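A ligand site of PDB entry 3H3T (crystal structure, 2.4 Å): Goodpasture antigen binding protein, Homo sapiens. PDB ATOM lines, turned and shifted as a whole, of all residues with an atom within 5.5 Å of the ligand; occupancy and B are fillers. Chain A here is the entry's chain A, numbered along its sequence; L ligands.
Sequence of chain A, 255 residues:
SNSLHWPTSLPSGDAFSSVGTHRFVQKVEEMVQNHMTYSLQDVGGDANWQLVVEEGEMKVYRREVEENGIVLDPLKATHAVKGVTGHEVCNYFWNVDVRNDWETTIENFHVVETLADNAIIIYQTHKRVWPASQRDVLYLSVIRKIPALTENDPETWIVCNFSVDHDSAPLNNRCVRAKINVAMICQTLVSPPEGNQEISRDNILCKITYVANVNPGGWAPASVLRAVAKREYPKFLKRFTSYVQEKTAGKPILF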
ATOM      1  N   PHE A  93      -4.860 -17.052 -21.331  1.00  0.00           N
ATOM      2  CA  PHE A  93      -6.221 -16.560 -21.398  1.00  0.00           C
ATOM      3  C   PHE A  93      -7.112 -17.585 -22.048  1.00  0.00           C
ATOM      4  O   PHE A  93      -8.226 -17.783 -21.610  1.00  0.00           O
ATOM      5  CB  PHE A  93      -6.321 -15.205 -22.136  1.00  0.00           C
ATOM      6  CG  PHE A  93      -7.739 -14.666 -22.180  1.00  0.00           C
ATOM      7  CD1 PHE A  93      -8.385 -14.298 -21.023  1.00  0.00           C
ATOM      8  CD2 PHE A  93      -8.420 -14.554 -23.370  1.00  0.00           C
ATOM      9  CE1 PHE A  93      -9.703 -13.836 -21.041  1.00  0.00           C
ATOM     10  CE2 PHE A  93      -9.731 -14.063 -23.391  1.00  0.00           C
ATOM     11  CZ  PHE A  93     -10.366 -13.711 -22.233  1.00  0.00           C
ATOM     12  N   ARG A  99      -8.327 -22.209 -16.593  1.00  0.00           N
ATOM     13  CA  ARG A  99      -9.368 -21.218 -16.326  1.00  0.00           C
ATOM     14  C   ARG A  99      -9.657 -21.030 -14.819  1.00  0.00           C
ATOM     15  O   ARG A  99      -9.696 -19.898 -14.307  1.00  0.00           O
ATOM     16  CB  ARG A  99     -10.634 -21.570 -17.102  1.00  0.00           C
ATOM     17  CG  ARG A  99     -11.804 -20.654 -16.788  1.00  0.00           C
ATOM     18  CD  ARG A  99     -12.235 -19.786 -17.977  1.00  0.00           C
ATOM     19  NE  ARG A  99     -11.148 -19.573 -18.905  1.00  0.00           N
ATOM     20  CZ  ARG A  99     -11.249 -19.684 -20.220  1.00  0.00           C
ATOM     21  NH1 ARG A  99     -10.177 -19.465 -20.976  1.00  0.00           N
ATOM     22  NH2 ARG A  99     -12.386 -19.990 -20.806  1.00  0.00           N
ATOM     23  N   TRP A 102      -7.655 -18.817 -12.414  1.00  0.00           N
ATOM     24  CA  TRP A 102      -7.728 -17.345 -12.358  1.00  0.00           C
ATOM     25  C   TRP A 102      -9.142 -16.792 -12.385  1.00  0.00           C
ATOM     26  O   TRP A 102      -9.395 -15.744 -11.816  1.00  0.00           O
ATOM     27  CB  TRP A 102      -6.854 -16.689 -13.440  1.00  0.00           C
ATOM     28  CG  TRP A 102      -7.236 -17.058 -14.846  1.00  0.00           C
ATOM     29  CD1 TRP A 102      -6.690 -18.030 -15.617  1.00  0.00           C
ATOM     30  CD2 TRP A 102      -8.285 -16.457 -15.622  1.00  0.00           C
ATOM     31  NE1 TRP A 102      -7.313 -18.073 -16.848  1.00  0.00           N
ATOM     32  CE2 TRP A 102      -8.290 -17.108 -16.875  1.00  0.00           C
ATOM     33  CE3 TRP A 102      -9.195 -15.425 -15.389  1.00  0.00           C
ATOM     34  CZ2 TRP A 102      -9.198 -16.770 -17.882  1.00  0.00           C
ATOM     35  CZ3 TRP A 102     -10.085 -15.087 -16.393  1.00  0.00           C
ATOM     36  CH2 TRP A 102     -10.065 -15.756 -17.628  1.00  0.00           C
ATOM     37  N   GLU A 103     -10.056 -17.492 -13.041  1.00  0.00           N
ATOM     38  CA  GLU A 103     -11.433 -17.014 -13.178  1.00  0.00           C
ATOM     39  C   GLU A 103     -12.230 -17.135 -11.864  1.00  0.00           C
ATOM     40  O   GLU A 103     -12.323 -18.215 -11.287  1.00  0.00           O
ATOM     41  CB  GLU A 103     -12.105 -17.758 -14.341  1.00  0.00           C
ATOM     42  CG  GLU A 103     -13.567 -17.463 -14.602  1.00  0.00           C
ATOM     43  CD  GLU A 103     -13.813 -16.055 -15.073  1.00  0.00           C
ATOM     44  OE1 GLU A 103     -13.731 -15.805 -16.299  1.00  0.00           O
ATOM     45  OE2 GLU A 103     -14.131 -15.203 -14.219  1.00  0.00           O
ATOM     46  N   THR A 105     -15.543 -15.563 -11.603  1.00  0.00           N
ATOM     47  CA  THR A 105     -16.951 -15.303 -11.842  1.00  0.00           C
ATOM     48  C   THR A 105     -17.715 -16.517 -12.378  1.00  0.00           C
ATOM     49  O   THR A 105     -18.927 -16.461 -12.555  1.00  0.00           O
ATOM     50  CB  THR A 105     -17.137 -14.099 -12.787  1.00  0.00           C
ATOM     51  OG1 THR A 105     -16.830 -14.476 -14.136  1.00  0.00           O
ATOM     52  CG2 THR A 105     -16.262 -12.958 -12.374  1.00  0.00           C
ATOM     53  N   ILE A 106     -17.027 -17.618 -12.626  1.00  0.00           N
ATOM     54  CA  ILE A 106     -17.627 -18.770 -13.268  1.00  0.00           C
ATOM     55  C   ILE A 106     -18.190 -19.760 -12.239  1.00  0.00           C
ATOM     56  O   ILE A 106     -17.601 -19.977 -11.188  1.00  0.00           O
ATOM     57  CB  ILE A 106     -16.607 -19.480 -14.177  1.00  0.00           C
ATOM     58  CG1 ILE A 106     -16.598 -18.835 -15.564  1.00  0.00           C
ATOM     59  CG2 ILE A 106     -16.954 -20.930 -14.372  1.00  0.00           C
ATOM     60  CD1 ILE A 106     -15.774 -19.611 -16.584  1.00  0.00           C
ATOM     61  N   GLN A 124     -20.857 -21.801 -20.493  1.00  0.00           N
ATOM     62  CA  GLN A 124     -20.597 -21.626 -19.082  1.00  0.00           C
ATOM     63  C   GLN A 124     -21.706 -20.863 -18.373  1.00  0.00           C
ATOM     64  O   GLN A 124     -22.465 -20.117 -18.996  1.00  0.00           O
ATOM     65  CB  GLN A 124     -19.254 -20.933 -18.877  1.00  0.00           C
ATOM     66  CG  GLN A 124     -19.230 -19.468 -19.187  1.00  0.00           C
ATOM     67  CD  GLN A 124     -17.809 -18.987 -19.309  1.00  0.00           C
ATOM     68  OE1 GLN A 124     -16.956 -19.725 -19.790  1.00  0.00           O
ATOM     69  NE2 GLN A 124     -17.538 -17.764 -18.870  1.00  0.00           N
ATOM     70  N   HIS A 126     -22.431 -18.280 -15.037  1.00  0.00           N
ATOM     71  CA  HIS A 126     -21.738 -17.384 -14.143  1.00  0.00           C
ATOM     72  C   HIS A 126     -22.353 -17.328 -12.752  1.00  0.00           C
ATOM     73  O   HIS A 126     -23.561 -17.526 -12.586  1.00  0.00           O
ATOM     74  CB  HIS A 126     -21.673 -15.984 -14.756  1.00  0.00           C
ATOM     75  CG  HIS A 126     -20.641 -15.851 -15.827  1.00  0.00           C
ATOM     76  ND1 HIS A 126     -19.361 -15.420 -15.561  1.00  0.00           N
ATOM     77  CD2 HIS A 126     -20.691 -16.133 -17.150  1.00  0.00           C
ATOM     78  CE1 HIS A 126     -18.668 -15.437 -16.687  1.00  0.00           C
ATOM     79  NE2 HIS A 126     -19.450 -15.862 -17.656  1.00  0.00           N
ATOM     80  N   LYS A 127     -21.504 -17.099 -11.753  1.00  0.00           N
ATOM     81  CA  LYS A 127     -21.964 -16.755 -10.409  1.00  0.00           C
ATOM     82  C   LYS A 127     -22.797 -15.474 -10.511  1.00  0.00           C
ATOM     83  O   LYS A 127     -22.634 -14.672 -11.444  1.00  0.00           O
ATOM     84  CB  LYS A 127     -20.795 -16.500  -9.452  1.00  0.00           C
ATOM     85  CG  LYS A 127     -19.678 -17.564  -9.423  1.00  0.00           C
ATOM     86  CD  LYS A 127     -18.676 -17.225  -8.295  1.00  0.00           C
ATOM     87  CE  LYS A 127     -17.598 -18.273  -8.098  1.00  0.00           C
ATOM     88  NZ  LYS A 127     -18.121 -19.515  -7.443  1.00  0.00           N
ATOM     89  N   VAL A 129     -23.336 -11.988 -10.028  1.00  0.00           N
ATOM     90  CA  VAL A 129     -22.534 -10.837  -9.629  1.00  0.00           C
ATOM     91  C   VAL A 129     -23.438  -9.653  -9.328  1.00  0.00           C
ATOM     92  O   VAL A 129     -23.004  -8.677  -8.723  1.00  0.00           O
ATOM     93  CB  VAL A 129     -21.439 -10.465 -10.669  1.00  0.00           C
ATOM     94  CG1 VAL A 129     -20.289 -11.456 -10.625  1.00  0.00           C
ATOM     95  CG2 VAL A 129     -22.032 -10.370 -12.038  1.00  0.00           C
ATOM     96  N   TRP A 130     -24.695  -9.733  -9.761  1.00  0.00           N
ATOM     97  CA  TRP A 130     -25.747  -8.979  -9.078  1.00  0.00           C
ATOM     98  C   TRP A 130     -26.870  -9.938  -8.666  1.00  0.00           C
ATOM     99  O   TRP A 130     -26.945 -11.064  -9.193  1.00  0.00           O
ATOM    100  CB  TRP A 130     -26.251  -7.773  -9.898  1.00  0.00           C
ATOM    101  CG  TRP A 130     -26.938  -8.106 -11.188  1.00  0.00           C
ATOM    102  CD1 TRP A 130     -28.296  -8.139 -11.411  1.00  0.00           C
ATOM    103  CD2 TRP A 130     -26.326  -8.426 -12.441  1.00  0.00           C
ATOM    104  NE1 TRP A 130     -28.542  -8.460 -12.727  1.00  0.00           N
ATOM    105  CE2 TRP A 130     -27.351  -8.642 -13.379  1.00  0.00           C
ATOM    106  CE3 TRP A 130     -24.990  -8.550 -12.869  1.00  0.00           C
ATOM    107  CZ2 TRP A 130     -27.095  -8.980 -14.705  1.00  0.00           C
ATOM    108  CZ3 TRP A 130     -24.734  -8.888 -14.195  1.00  0.00           C
ATOM    109  CH2 TRP A 130     -25.790  -9.099 -15.096  1.00  0.00           C
ATOM    110  N   ARG A 135     -26.504 -15.617 -15.210  1.00  0.00           N
ATOM    111  CA  ARG A 135     -26.394 -15.525 -16.650  1.00  0.00           C
ATOM    112  C   ARG A 135     -25.557 -16.687 -17.093  1.00  0.00           C
ATOM    113  O   ARG A 135     -24.634 -17.084 -16.378  1.00  0.00           O
ATOM    114  CB  ARG A 135     -25.659 -14.250 -17.034  1.00  0.00           C
ATOM    115  CG  ARG A 135     -26.581 -13.136 -17.418  1.00  0.00           C
ATOM    116  CD  ARG A 135     -27.409 -12.639 -16.254  1.00  0.00           C
ATOM    117  NE  ARG A 135     -28.361 -11.658 -16.738  1.00  0.00           N
ATOM    118  CZ  ARG A 135     -29.441 -11.241 -16.090  1.00  0.00           C
ATOM    119  NH1 ARG A 135     -29.728 -11.719 -14.886  1.00  0.00           N
ATOM    120  NH2 ARG A 135     -30.233 -10.347 -16.645  1.00  0.00           N
ATOM    121  N   VAL A 137     -23.537 -18.204 -20.840  1.00  0.00           N
ATOM    122  CA  VAL A 137     -23.015 -17.711 -22.096  1.00  0.00           C
ATOM    123  C   VAL A 137     -22.540 -18.858 -22.965  1.00  0.00           C
ATOM    124  O   VAL A 137     -22.069 -19.866 -22.464  1.00  0.00           O
ATOM    125  CB  VAL A 137     -21.893 -16.661 -21.869  1.00  0.00           C
ATOM    126  CG1 VAL A 137     -20.795 -17.225 -21.014  1.00  0.00           C
ATOM    127  CG2 VAL A 137     -21.341 -16.163 -23.214  1.00  0.00           C
ATOM    128  N   TYR A 139     -20.107 -19.258 -26.198  1.00  0.00           N
ATOM    129  CA  TYR A 139     -19.202 -18.526 -27.078  1.00  0.00           C
ATOM    130  C   TYR A 139     -18.081 -19.339 -27.702  1.00  0.00           C
ATOM    131  O   TYR A 139     -17.595 -20.298 -27.120  1.00  0.00           O
ATOM    132  CB  TYR A 139     -18.564 -17.357 -26.354  1.00  0.00           C
ATOM    133  CG  TYR A 139     -17.682 -17.793 -25.202  1.00  0.00           C
ATOM    134  CD1 TYR A 139     -16.302 -17.692 -25.264  1.00  0.00           C
ATOM    135  CD2 TYR A 139     -18.232 -18.308 -24.040  1.00  0.00           C
ATOM    136  CE1 TYR A 139     -15.522 -18.093 -24.216  1.00  0.00           C
ATOM    137  CE2 TYR A 139     -17.455 -18.686 -22.976  1.00  0.00           C
ATOM    138  CZ  TYR A 139     -16.105 -18.594 -23.067  1.00  0.00           C
ATOM    139  OH  TYR A 139     -15.315 -18.987 -21.979  1.00  0.00           O
ATOM    140  N   ASN A 161     -13.493 -13.987 -28.027  1.00  0.00           N
ATOM    141  CA  ASN A 161     -14.596 -14.743 -27.429  1.00  0.00           C
ATOM    142  C   ASN A 161     -15.854 -14.034 -27.879  1.00  0.00           C
ATOM    143  O   ASN A 161     -16.057 -12.874 -27.520  1.00  0.00           O
ATOM    144  CB  ASN A 161     -14.525 -14.671 -25.906  1.00  0.00           C
ATOM    145  CG  ASN A 161     -13.412 -15.537 -25.334  1.00  0.00           C
ATOM    146  OD1 ASN A 161     -12.939 -15.297 -24.221  1.00  0.00           O
ATOM    147  ND2 ASN A 161     -12.991 -16.547 -26.098  1.00  0.00           N
ATOM    148  N   ALA A 178     -26.615 -14.161 -21.841  1.00  0.00           N
ATOM    149  CA  ALA A 178     -25.786 -13.027 -22.207  1.00  0.00           C
ATOM    150  C   ALA A 178     -25.157 -13.279 -23.565  1.00  0.00           C
ATOM    151  O   ALA A 178     -24.926 -14.420 -23.946  1.00  0.00           O
ATOM    152  CB  ALA A 178     -24.714 -12.812 -21.150  1.00  0.00           C
ATOM    153  N   ILE A 180     -21.780 -11.962 -25.788  1.00  0.00           N
ATOM    154  CA  ILE A 180     -20.523 -11.258 -25.651  1.00  0.00           C
ATOM    155  C   ILE A 180     -19.778 -11.076 -26.961  1.00  0.00           C
ATOM    156  O   ILE A 180     -19.960 -11.815 -27.925  1.00  0.00           O
ATOM    157  CB  ILE A 180     -19.582 -11.963 -24.639  1.00  0.00           C
ATOM    158  CG1 ILE A 180     -19.389 -13.445 -24.977  1.00  0.00           C
ATOM    159  CG2 ILE A 180     -20.124 -11.857 -23.257  1.00  0.00           C
ATOM    160  CD1 ILE A 180     -18.236 -14.144 -24.205  1.00  0.00           C
ATOM    161  N   VAL A 182     -15.701 -10.228 -26.992  1.00  0.00           N
ATOM    162  CA  VAL A 182     -14.562  -9.924 -26.145  1.00  0.00           C
ATOM    163  C   VAL A 182     -13.290 -10.164 -26.946  1.00  0.00           C
ATOM    164  O   VAL A 182     -13.239 -11.055 -27.793  1.00  0.00           O
ATOM    165  CB  VAL A 182     -14.548 -10.812 -24.867  1.00  0.00           C
ATOM    166  CG1 VAL A 182     -13.290 -10.584 -24.004  1.00  0.00           C
ATOM    167  CG2 VAL A 182     -15.815 -10.616 -24.040  1.00  0.00           C
ATOM    168  N   TYR A 210      -7.624  -5.126 -23.791  1.00  0.00           N
ATOM    169  CA  TYR A 210      -8.750  -6.019 -23.567  1.00  0.00           C
ATOM    170  C   TYR A 210     -10.034  -5.223 -23.753  1.00  0.00           C
ATOM    171  O   TYR A 210     -10.259  -4.201 -23.058  1.00  0.00           O
ATOM    172  CB  TYR A 210      -8.711  -6.568 -22.146  1.00  0.00           C
ATOM    173  CG  TYR A 210      -9.943  -7.370 -21.702  1.00  0.00           C
ATOM    174  CD1 TYR A 210     -11.003  -6.769 -21.052  1.00  0.00           C
ATOM    175  CD2 TYR A 210     -10.003  -8.732 -21.911  1.00  0.00           C
ATOM    176  CE1 TYR A 210     -12.125  -7.509 -20.652  1.00  0.00           C
ATOM    177  CE2 TYR A 210     -11.093  -9.485 -21.498  1.00  0.00           C
ATOM    178  CZ  TYR A 210     -12.146  -8.868 -20.881  1.00  0.00           C
ATOM    179  OH  TYR A 210     -13.230  -9.629 -20.468  1.00  0.00           O
ATOM    180  N   ALA A 212     -14.385  -5.516 -24.044  1.00  0.00           N
ATOM    181  CA  ALA A 212     -15.524  -6.355 -23.752  1.00  0.00           C
ATOM    182  C   ALA A 212     -16.788  -5.587 -24.103  1.00  0.00           C
ATOM    183  O   ALA A 212     -17.011  -4.485 -23.617  1.00  0.00           O
ATOM    184  CB  ALA A 212     -15.516  -6.816 -22.313  1.00  0.00           C
ATOM    185  N   VAL A 214     -20.619  -6.511 -23.777  1.00  0.00           N
ATOM    186  CA  VAL A 214     -21.536  -7.518 -23.249  1.00  0.00           C
ATOM    187  C   VAL A 214     -22.979  -7.030 -23.202  1.00  0.00           C
ATOM    188  O   VAL A 214     -23.271  -5.905 -22.749  1.00  0.00           O
ATOM    189  CB  VAL A 214     -21.124  -7.943 -21.827  1.00  0.00           C
ATOM    190  CG1 VAL A 214     -22.189  -8.830 -21.199  1.00  0.00           C
ATOM    191  CG2 VAL A 214     -19.757  -8.616 -21.837  1.00  0.00           C
ATOM    192  N   PRO A 216     -26.065  -8.131 -21.268  1.00  0.00           N
ATOM    193  CA  PRO A 216     -26.479  -8.879 -20.075  1.00  0.00           C
ATOM    194  C   PRO A 216     -27.745  -9.713 -20.300  1.00  0.00           C
ATOM    195  O   PRO A 216     -28.035 -10.581 -19.479  1.00  0.00           O
ATOM    196  CB  PRO A 216     -26.742  -7.788 -19.032  1.00  0.00           C
ATOM    197  CG  PRO A 216     -26.898  -6.557 -19.765  1.00  0.00           C
ATOM    198  CD  PRO A 216     -26.151  -6.676 -21.057  1.00  0.00           C
ATOM    199  N   VAL A 228     -20.725  -3.072 -10.983  1.00  0.00           N
ATOM    200  CA  VAL A 228     -20.199  -4.416 -11.116  1.00  0.00           C
ATOM    201  C   VAL A 228     -19.093  -4.487 -12.193  1.00  0.00           C
ATOM    202  O   VAL A 228     -18.049  -5.083 -11.961  1.00  0.00           O
ATOM    203  CB  VAL A 228     -21.354  -5.453 -11.355  1.00  0.00           C
ATOM    204  CG1 VAL A 228     -20.809  -6.792 -11.760  1.00  0.00           C
ATOM    205  CG2 VAL A 228     -22.204  -5.599 -10.076  1.00  0.00           C
ATOM    206  N   ALA A 229     -19.273  -3.832 -13.333  1.00  0.00           N
ATOM    207  CA  ALA A 229     -18.236  -3.816 -14.350  1.00  0.00           C
ATOM    208  C   ALA A 229     -16.987  -3.189 -13.765  1.00  0.00           C
ATOM    209  O   ALA A 229     -15.906  -3.770 -13.865  1.00  0.00           O
ATOM    210  CB  ALA A 229     -18.682  -3.056 -15.597  1.00  0.00           C
ATOM    211  N   GLU A 232     -15.408  -5.740 -11.236  1.00  0.00           N
ATOM    212  CA  GLU A 232     -14.995  -7.073 -11.659  1.00  0.00           C
ATOM    213  C   GLU A 232     -13.955  -7.106 -12.789  1.00  0.00           C
ATOM    214  O   GLU A 232     -13.126  -7.994 -12.834  1.00  0.00           O
ATOM    215  CB  GLU A 232     -16.213  -7.880 -12.097  1.00  0.00           C
ATOM    216  CG  GLU A 232     -17.133  -8.275 -10.960  1.00  0.00           C
ATOM    217  CD  GLU A 232     -16.445  -9.152  -9.908  1.00  0.00           C
ATOM    218  OE1 GLU A 232     -15.792 -10.172 -10.264  1.00  0.00           O
ATOM    219  OE2 GLU A 232     -16.563  -8.832  -8.716  1.00  0.00           O
ATOM    220  N   TYR A 233     -13.988  -6.148 -13.693  1.00  0.00           N
ATOM    221  CA  TYR A 233     -12.988  -6.159 -14.764  1.00  0.00           C
ATOM    222  C   TYR A 233     -11.562  -5.923 -14.273  1.00  0.00           C
ATOM    223  O   TYR A 233     -10.678  -6.695 -14.556  1.00  0.00           O
ATOM    224  CB  TYR A 233     -13.366  -5.215 -15.891  1.00  0.00           C
ATOM    225  CG  TYR A 233     -14.470  -5.762 -16.757  1.00  0.00           C
ATOM    226  CD1 TYR A 233     -14.200  -6.700 -17.732  1.00  0.00           C
ATOM    227  CD2 TYR A 233     -15.783  -5.339 -16.597  1.00  0.00           C
ATOM    228  CE1 TYR A 233     -15.207  -7.202 -18.523  1.00  0.00           C
ATOM    229  CE2 TYR A 233     -16.788  -5.828 -17.394  1.00  0.00           C
ATOM    230  CZ  TYR A 233     -16.486  -6.756 -18.353  1.00  0.00           C
ATOM    231  OH  TYR A 233     -17.480  -7.236 -19.147  1.00  0.00           O
ATOM    232  N   PHE A 236     -10.340  -8.934 -12.335  1.00  0.00           N
ATOM    233  CA  PHE A 236      -9.939  -9.975 -13.265  1.00  0.00           C
ATOM    234  C   PHE A 236      -8.583  -9.666 -13.904  1.00  0.00           C
ATOM    235  O   PHE A 236      -7.714 -10.525 -13.946  1.00  0.00           O
ATOM    236  CB  PHE A 236     -11.027 -10.177 -14.331  1.00  0.00           C
ATOM    237  CG  PHE A 236     -10.509 -10.374 -15.749  1.00  0.00           C
ATOM    238  CD1 PHE A 236      -9.785 -11.513 -16.096  1.00  0.00           C
ATOM    239  CD2 PHE A 236     -10.764  -9.425 -16.728  1.00  0.00           C
ATOM    240  CE1 PHE A 236      -9.327 -11.700 -17.417  1.00  0.00           C
ATOM    241  CE2 PHE A 236     -10.317  -9.595 -18.049  1.00  0.00           C
ATOM    242  CZ  PHE A 236      -9.583 -10.739 -18.387  1.00  0.00           C
HETATM  243  O1  LIG L   1     -13.109 -12.554 -20.220  1.00  0.00           O
HETATM  244  C1  LIG L   1     -13.328 -13.197 -19.202  1.00  0.00           C
HETATM  245  N1  LIG L   1     -13.730 -14.470 -19.128  1.00  0.00           N
HETATM  246  C2  LIG L   1     -13.800 -15.429 -20.231  1.00  0.00           C
HETATM  247  C3  LIG L   1     -13.485 -16.863 -19.785  1.00  0.00           C
HETATM  248  O2  LIG L   1     -14.250 -17.259 -18.631  1.00  0.00           O
HETATM  249  C4  LIG L   1     -15.168 -15.325 -20.928  1.00  0.00           C
HETATM  250  C5  LIG L   1     -15.123 -13.832 -21.223  1.00  0.00           C
HETATM  251  C6  LIG L   1     -16.231 -13.012 -20.668  1.00  0.00           C
HETATM  252  C7  LIG L   1     -17.350 -13.598 -20.091  1.00  0.00           C
HETATM  253  C8  LIG L   1     -18.303 -12.756 -19.539  1.00  0.00           C
HETATM  254  C9  LIG L   1     -18.157 -11.365 -19.527  1.00  0.00           C
HETATM  255  C10 LIG L   1     -17.020 -10.791 -20.073  1.00  0.00           C
HETATM  256  C11 LIG L   1     -16.074 -11.637 -20.620  1.00  0.00           C
HETATM  257  O3  LIG L   1     -14.574 -13.467 -22.481  1.00  0.00           O
HETATM  258  C12 LIG L   1     -13.097 -12.498 -17.892  1.00  0.00           C
HETATM  259  C13 LIG L   1     -14.325 -11.727 -17.446  1.00  0.00           C
HETATM  260  C14 LIG L   1     -14.086 -11.250 -16.020  1.00  0.00           C
HETATM  261  C15 LIG L   1     -14.920 -10.018 -15.736  1.00  0.00           C
HETATM  262  C16 LIG L   1     -16.374 -10.459 -15.566  1.00  0.00           C
HETATM  263  C17 LIG L   1     -17.320  -9.323 -15.887  1.00  0.00           C
HETATM  264  C18 LIG L   1     -18.482  -9.354 -14.897  1.00  0.00           C
HETATM  265  C19 LIG L   1     -19.686  -8.549 -15.399  1.00  0.00           C
HETATM  266  C20 LIG L   1     -20.931  -9.435 -15.438  1.00  0.00           C
HETATM  267  C21 LIG L   1     -20.549 -10.915 -15.600  1.00  0.00           C
HETATM  268  C22 LIG L   1     -21.745 -11.852 -15.620  1.00  0.00           C
HETATM  269  C23 LIG L   1     -22.918 -11.202 -16.328  1.00  0.00           C
HETATM  270  C24 LIG L   1     -22.590 -10.947 -17.787  1.00  0.00           C
HETATM  271  C25 LIG L   1     -22.464 -12.293 -18.485  1.00  0.00           C
HETATM  272  C26 LIG L   1     -21.633 -12.146 -19.732  1.00  0.00           C
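Phe 93 touches the ligand (CZ to O1, 3.6 Å). CD of Arg 99 touches O2 of the ligand (3.3 Å). Ile 106 touches the ligand. NE2 of His 126 touches C8 of the ligand (3.8 Å). CG2 of Val 129 touches C20 of the ligand, at 3.7 Å. Trp 130 touches the ligand. OH of Tyr 139 touches C3 of the ligand, at 3.6 Å. CB of Ala 178 touches C26 of the ligand, 3.5 Å away. CG2 of Ile 180 touches C26 of the ligand (3.8 Å). CG2 of Val 182 touches O3 of the ligand, at 3.5 Å. Val 214 touches the ligand. CB of Glu 232 touches C18 of the ligand, 3.9 Å away. Tyr 233 touches the ligand. Phe 236 touches the ligand. Hydrophobic or aromatic side chains that line the ligand: Phe 93, Ile 106, His 126, Val 129, Trp 130, Ala 178, Ile 180, Val 182, Tyr 210, Val 214, Tyr 233 and Phe 236. 18 residues have an atom within 4 Å of the ligand: Phe 93, Arg 99, Glu 103, Ile 106, Gln 124, His 126, Val 129, Trp 130, Tyr 139, Asn 161, Ala 178, Ile 180, Val 182, Tyr 210, Val 214, Glu 232, Tyr 233 and Phe 236.
An oxygen (O2) of the ligand sits at hydrogen-bond distance from the side-chain carboxylate (OE1) of Glu 103 (2.8 Å). The side-chain hydroxyl of Tyr 210 is in hydrogen-bond range of an oxygen (O1) of the ligand, at 2.9 Å. The side-chain amide oxygen of Asn 161 lies within hydrogen-bond range of an oxygen (O3) of the ligand, 3.0 Å away. An oxygen (O2) of the ligand sits at hydrogen-bond distance from the side-chain amide nitrogen (NE2) of Gln 124 (3.3 Å).
The side-chain carboxylate (OE2) of Glu 103 is in hydrogen-bond range of the side-chain hydroxyl (OG1) of Thr 105. The guanidinium group (NH2) of Arg 99 sits at hydrogen-bond distance from the side-chain hydroxyl (OH) of Tyr 139 (3.3 Å). NH1 of Arg 99 sits at hydrogen-bond distance from O of Phe 93, at 2.7 Å. OE1 of Gln 124 sits at hydrogen-bond distance from OH of Tyr 139 (2.8 Å). NE2 of Gln 124 lies within hydrogen-bond range of NE2 of His 126. The backbone NH (N) of Val 137 lies within hydrogen-bond range of the backbone carbonyl oxygen (O) of Gln 124, at 2.9 Å. N of His 126 is in hydrogen-bond range of O of Arg 135, 2.8 Å away. The side-chain hydroxyl (OG1) of Thr 105 sits at hydrogen-bond distance from a ring nitrogen (ND1) of His 126, 3.1 Å away.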
